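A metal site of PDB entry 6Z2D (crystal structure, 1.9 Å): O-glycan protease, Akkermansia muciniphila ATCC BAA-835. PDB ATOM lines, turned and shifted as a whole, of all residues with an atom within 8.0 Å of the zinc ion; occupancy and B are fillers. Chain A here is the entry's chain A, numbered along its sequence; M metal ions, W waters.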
ATOM      1  N   TYR A 143     -13.874  -3.689 -37.509  1.00  0.00           N
ATOM      2  CA  TYR A 143     -13.205  -2.637 -36.719  1.00  0.00           C
ATOM      3  C   TYR A 143     -13.989  -1.333 -36.870  1.00  0.00           C
ATOM      4  O   TYR A 143     -14.819  -1.196 -37.704  1.00  0.00           O
ATOM      5  CB  TYR A 143     -11.799  -2.354 -37.255  1.00  0.00           C
ATOM      6  CG  TYR A 143     -11.525  -2.616 -38.725  1.00  0.00           C
ATOM      7  CD1 TYR A 143     -12.037  -1.814 -39.717  1.00  0.00           C
ATOM      8  CD2 TYR A 143     -10.833  -3.739 -39.123  1.00  0.00           C
ATOM      9  CE1 TYR A 143     -11.822  -2.099 -41.046  1.00  0.00           C
ATOM     10  CE2 TYR A 143     -10.606  -4.030 -40.448  1.00  0.00           C
ATOM     11  CZ  TYR A 143     -11.111  -3.210 -41.416  1.00  0.00           C
ATOM     12  OH  TYR A 143     -10.895  -3.463 -42.727  1.00  0.00           O
ATOM     13  N   GLY A 144     -13.695  -0.395 -35.977  1.00  0.00           N
ATOM     14  CA  GLY A 144     -14.165   0.961 -36.177  1.00  0.00           C
ATOM     15  C   GLY A 144     -13.277   1.702 -37.155  1.00  0.00           C
ATOM     16  O   GLY A 144     -12.071   1.504 -37.207  1.00  0.00           O
ATOM     17  N   GLY A 178     -18.659  -8.500 -30.153  1.00  0.00           N
ATOM     18  CA  GLY A 178     -17.767  -7.787 -31.051  1.00  0.00           C
ATOM     19  C   GLY A 178     -18.455  -6.656 -31.781  1.00  0.00           C
ATOM     20  O   GLY A 178     -17.935  -5.537 -31.855  1.00  0.00           O
ATOM     21  N   HIS A 181     -19.142  -3.727 -29.488  1.00  0.00           N
ATOM     22  CA  HIS A 181     -17.936  -2.966 -29.164  1.00  0.00           C
ATOM     23  C   HIS A 181     -17.495  -2.133 -30.359  1.00  0.00           C
ATOM     24  O   HIS A 181     -17.134  -0.960 -30.200  1.00  0.00           O
ATOM     25  CB  HIS A 181     -16.848  -3.952 -28.728  1.00  0.00           C
ATOM     26  CG  HIS A 181     -15.495  -3.335 -28.487  1.00  0.00           C
ATOM     27  ND1 HIS A 181     -14.944  -3.236 -27.227  1.00  0.00           N
ATOM     28  CD2 HIS A 181     -14.562  -2.865 -29.350  1.00  0.00           C
ATOM     29  CE1 HIS A 181     -13.745  -2.686 -27.316  1.00  0.00           C
ATOM     30  NE2 HIS A 181     -13.477  -2.466 -28.589  1.00  0.00           N
ATOM     31  N   GLU A 182     -17.497  -2.719 -31.562  1.00  0.00           N
ATOM     32  CA  GLU A 182     -17.104  -1.954 -32.743  1.00  0.00           C
ATOM     33  C   GLU A 182     -18.101  -0.841 -33.019  1.00  0.00           C
ATOM     34  O   GLU A 182     -17.711   0.246 -33.457  1.00  0.00           O
ATOM     35  CB  GLU A 182     -16.999  -2.856 -33.977  1.00  0.00           C
ATOM     36  CG  GLU A 182     -16.061  -4.035 -33.825  1.00  0.00           C
ATOM     37  CD  GLU A 182     -14.602  -3.659 -33.543  1.00  0.00           C
ATOM     38  OE1 GLU A 182     -14.202  -2.508 -33.781  1.00  0.00           O
ATOM     39  OE2 GLU A 182     -13.864  -4.556 -33.087  1.00  0.00           O
ATOM     40  N   GLY A 184     -19.619   0.768 -30.751  1.00  0.00           N
ATOM     41  CA  GLY A 184     -19.242   1.820 -29.820  1.00  0.00           C
ATOM     42  C   GLY A 184     -18.169   2.720 -30.393  1.00  0.00           C
ATOM     43  O   GLY A 184     -18.277   3.946 -30.340  1.00  0.00           O
ATOM     44  N   HIS A 185     -17.117   2.121 -30.977  1.00  0.00           N
ATOM     45  CA  HIS A 185     -16.092   2.894 -31.672  1.00  0.00           C
ATOM     46  C   HIS A 185     -16.709   3.763 -32.760  1.00  0.00           C
ATOM     47  O   HIS A 185     -16.382   4.954 -32.870  1.00  0.00           O
ATOM     48  CB  HIS A 185     -15.052   1.958 -32.288  1.00  0.00           C
ATOM     49  CG  HIS A 185     -14.118   1.342 -31.302  1.00  0.00           C
ATOM     50  ND1 HIS A 185     -13.588   2.037 -30.232  1.00  0.00           N
ATOM     51  CD2 HIS A 185     -13.604   0.082 -31.218  1.00  0.00           C
ATOM     52  CE1 HIS A 185     -12.803   1.240 -29.538  1.00  0.00           C
ATOM     53  NE2 HIS A 185     -12.781   0.047 -30.112  1.00  0.00           N
ATOM     54  N   LEU A 189     -16.676   6.163 -29.360  1.00  0.00           N
ATOM     55  CA  LEU A 189     -16.215   5.747 -28.033  1.00  0.00           C
ATOM     56  C   LEU A 189     -14.781   5.206 -28.095  1.00  0.00           C
ATOM     57  O   LEU A 189     -14.490   4.351 -28.940  1.00  0.00           O
ATOM     58  CB  LEU A 189     -17.142   4.676 -27.450  1.00  0.00           C
ATOM     59  CG  LEU A 189     -18.624   5.043 -27.234  1.00  0.00           C
ATOM     60  CD1 LEU A 189     -19.335   3.969 -26.396  1.00  0.00           C
ATOM     61  CD2 LEU A 189     -18.693   6.363 -26.510  1.00  0.00           C
ATOM     62  N   PRO A 190     -13.883   5.656 -27.223  1.00  0.00           N
ATOM     63  CA  PRO A 190     -12.579   5.001 -27.060  1.00  0.00           C
ATOM     64  C   PRO A 190     -12.726   3.828 -26.100  1.00  0.00           C
ATOM     65  O   PRO A 190     -13.784   3.598 -25.526  1.00  0.00           O
ATOM     66  CB  PRO A 190     -11.717   6.103 -26.458  1.00  0.00           C
ATOM     67  CG  PRO A 190     -12.696   6.830 -25.563  1.00  0.00           C
ATOM     68  CD  PRO A 190     -14.029   6.805 -26.310  1.00  0.00           C
ATOM     69  N   HIS A 191     -11.633   3.095 -25.903  1.00  0.00           N
ATOM     70  CA  HIS A 191     -11.608   2.058 -24.870  1.00  0.00           C
ATOM     71  C   HIS A 191     -11.620   2.665 -23.479  1.00  0.00           C
ATOM     72  O   HIS A 191     -11.119   3.791 -23.267  1.00  0.00           O
ATOM     73  CB  HIS A 191     -10.363   1.180 -25.025  1.00  0.00           C
ATOM     74  CG  HIS A 191     -10.336   0.394 -26.299  1.00  0.00           C
ATOM     75  ND1 HIS A 191      -9.201   0.275 -27.077  1.00  0.00           N
ATOM     76  CD2 HIS A 191     -11.307  -0.298 -26.934  1.00  0.00           C
ATOM     77  CE1 HIS A 191      -9.479  -0.463 -28.139  1.00  0.00           C
ATOM     78  NE2 HIS A 191     -10.750  -0.823 -28.073  1.00  0.00           N
ATOM     79  N   ASN A 192     -12.169   1.927 -22.505  1.00  0.00           N
ATOM     80  CA  ASN A 192     -11.989   2.354 -21.125  1.00  0.00           C
ATOM     81  C   ASN A 192     -12.270   1.191 -20.197  1.00  0.00           C
ATOM     82  O   ASN A 192     -12.859   0.182 -20.588  1.00  0.00           O
ATOM     83  CB  ASN A 192     -12.849   3.581 -20.744  1.00  0.00           C
ATOM     84  CG  ASN A 192     -14.366   3.323 -20.797  1.00  0.00           C
ATOM     85  OD1 ASN A 192     -14.827   2.241 -21.181  1.00  0.00           O
ATOM     86  ND2 ASN A 192     -15.129   4.311 -20.347  1.00  0.00           N
ATOM     87  N   LEU A 206     -18.395  -2.244 -21.622  1.00  0.00           N
ATOM     88  CA  LEU A 206     -18.456  -2.705 -23.003  1.00  0.00           C
ATOM     89  C   LEU A 206     -17.214  -2.299 -23.775  1.00  0.00           C
ATOM     90  O   LEU A 206     -16.666  -3.091 -24.555  1.00  0.00           O
ATOM     91  CB  LEU A 206     -19.714  -2.169 -23.700  1.00  0.00           C
ATOM     92  CG  LEU A 206     -19.767  -2.451 -25.196  1.00  0.00           C
ATOM     93  CD1 LEU A 206     -19.806  -3.963 -25.468  1.00  0.00           C
ATOM     94  CD2 LEU A 206     -20.956  -1.740 -25.845  1.00  0.00           C
ATOM     95  N   MET A 207     -16.749  -1.054 -23.597  1.00  0.00           N
ATOM     96  CA  MET A 207     -15.588  -0.609 -24.349  1.00  0.00           C
ATOM     97  C   MET A 207     -14.259  -1.010 -23.703  1.00  0.00           C
ATOM     98  O   MET A 207     -13.200  -0.543 -24.132  1.00  0.00           O
ATOM     99  CB  MET A 207     -15.649   0.916 -24.541  1.00  0.00           C
ATOM    100  CG  MET A 207     -16.877   1.354 -25.352  1.00  0.00           C
ATOM    101  SD  MET A 207     -17.152   0.380 -26.859  1.00  0.00           S
ATOM    102  CE  MET A 207     -15.622   0.676 -27.753  1.00  0.00           C
ATOM    103  N   GLY A 208     -14.301  -1.848 -22.672  1.00  0.00           N
ATOM    104  CA  GLY A 208     -13.092  -2.453 -22.149  1.00  0.00           C
ATOM    105  C   GLY A 208     -12.971  -3.862 -22.671  1.00  0.00           C
ATOM    106  O   GLY A 208     -12.602  -4.085 -23.827  1.00  0.00           O
ATOM    107  N   ASN A 211     -16.695  -6.878 -24.917  1.00  0.00           N
ATOM    108  CA  ASN A 211     -16.957  -7.674 -26.109  1.00  0.00           C
ATOM    109  C   ASN A 211     -16.763  -9.156 -25.839  1.00  0.00           C
ATOM    110  O   ASN A 211     -17.216  -9.977 -26.650  1.00  0.00           O
ATOM    111  CB  ASN A 211     -16.070  -7.223 -27.280  1.00  0.00           C
ATOM    112  CG  ASN A 211     -14.594  -7.126 -26.905  1.00  0.00           C
ATOM    113  OD1 ASN A 211     -14.220  -7.071 -25.739  1.00  0.00           O
ATOM    114  ND2 ASN A 211     -13.744  -7.108 -27.933  1.00  0.00           N
ATOM    115  N   VAL A 290      -3.757   3.522 -29.127  1.00  0.00           N
ATOM    116  CA  VAL A 290      -5.218   3.413 -29.134  1.00  0.00           C
ATOM    117  C   VAL A 290      -5.729   1.986 -28.984  1.00  0.00           C
ATOM    118  O   VAL A 290      -6.953   1.790 -28.876  1.00  0.00           O
ATOM    119  CB  VAL A 290      -5.806   4.032 -30.416  1.00  0.00           C
ATOM    120  N   ASN A 291      -4.849   0.976 -29.000  1.00  0.00           N
ATOM    121  CA  ASN A 291      -5.255  -0.387 -28.678  1.00  0.00           C
ATOM    122  C   ASN A 291      -4.377  -0.970 -27.572  1.00  0.00           C
ATOM    123  O   ASN A 291      -4.210  -2.187 -27.469  1.00  0.00           O
ATOM    124  CB  ASN A 291      -5.244  -1.289 -29.907  1.00  0.00           C
ATOM    125  CG  ASN A 291      -6.631  -1.429 -30.516  1.00  0.00           C
ATOM    126  OD1 ASN A 291      -7.225  -2.510 -30.503  1.00  0.00           O
ATOM    127  ND2 ASN A 291      -7.157  -0.320 -31.030  1.00  0.00           N
ATOM    128  N   ASP A 293      -4.964   0.699 -24.517  1.00  0.00           N
ATOM    129  CA  ASP A 293      -5.681   1.531 -23.559  1.00  0.00           C
ATOM    130  C   ASP A 293      -6.977   0.875 -23.069  1.00  0.00           C
ATOM    131  O   ASP A 293      -7.841   1.575 -22.537  1.00  0.00           O
ATOM    132  CB  ASP A 293      -5.992   2.896 -24.164  1.00  0.00           C
ATOM    133  CG  ASP A 293      -6.775   2.788 -25.465  1.00  0.00           C
ATOM    134  OD1 ASP A 293      -6.920   1.662 -26.000  1.00  0.00           O
ATOM    135  OD2 ASP A 293      -7.225   3.838 -25.969  1.00  0.00           O
ATOM    136  N   TYR A 294      -7.137  -0.449 -23.246  1.00  0.00           N
ATOM    137  CA  TYR A 294      -8.240  -1.139 -22.588  1.00  0.00           C
ATOM    138  C   TYR A 294      -8.195  -0.954 -21.090  1.00  0.00           C
ATOM    139  O   TYR A 294      -9.208  -1.155 -20.406  1.00  0.00           O
ATOM    140  CB  TYR A 294      -8.212  -2.636 -22.907  1.00  0.00           C
ATOM    141  CG  TYR A 294      -8.254  -2.947 -24.381  1.00  0.00           C
ATOM    142  CD1 TYR A 294      -9.472  -3.041 -25.058  1.00  0.00           C
ATOM    143  CD2 TYR A 294      -7.078  -3.143 -25.106  1.00  0.00           C
ATOM    144  CE1 TYR A 294      -9.514  -3.324 -26.416  1.00  0.00           C
ATOM    145  CE2 TYR A 294      -7.103  -3.423 -26.458  1.00  0.00           C
ATOM    146  CZ  TYR A 294      -8.323  -3.518 -27.113  1.00  0.00           C
ATOM    147  OH  TYR A 294      -8.357  -3.805 -28.452  1.00  0.00           O
HETATM  148 ZN    ZN M   1     -11.837  -1.708 -29.560  1.00  0.00          ZN
HETATM  149  O   HOH W   1     -12.074  -2.936 -31.498  1.00  0.00           O
HETATM  150  O   HOH W   2     -10.042  -1.405 -31.169  1.00  0.00           O
HETATM  151  O   HOH W   3     -10.557  -3.594 -29.652  1.00  0.00           O
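A ring nitrogen (ND1) of His 191 sits at hydrogen-bond distance from the backbone carbonyl oxygen of Val 290 (3.3 Å).
ND1 of His 191 lies within hydrogen-bond range of OD1 of Asp 293, at 2.9 Å.
The backbone carbonyl oxygen of Leu 206 sits at hydrogen-bond distance from a ring nitrogen (ND1) of His 181 (3.2 Å).
A ring nitrogen (ND1) of His 185 is in hydrogen-bond range of the backbone carbonyl oxygen (O) of Leu 189, 2.8 Å away.
Of the 19 residues printed, 3 come within 4 Å of the zinc ion.
The nearest printed residue that does not touch the zinc ion is Tyr 294 (4.2 Å).
NE2 of His 191 binds the zinc ion (2.0 Å).
The zinc ion is bound by NE2 of His 181, at 2.1 Å.
NE2 of His 185 binds the zinc ion, 2.1 Å away.
Water W3 is bound to the zinc ion.
Water W1 binds the zinc ion.
Water W2 is bound to the zinc ion.
The zinc ion has six donor atoms within binding distance.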
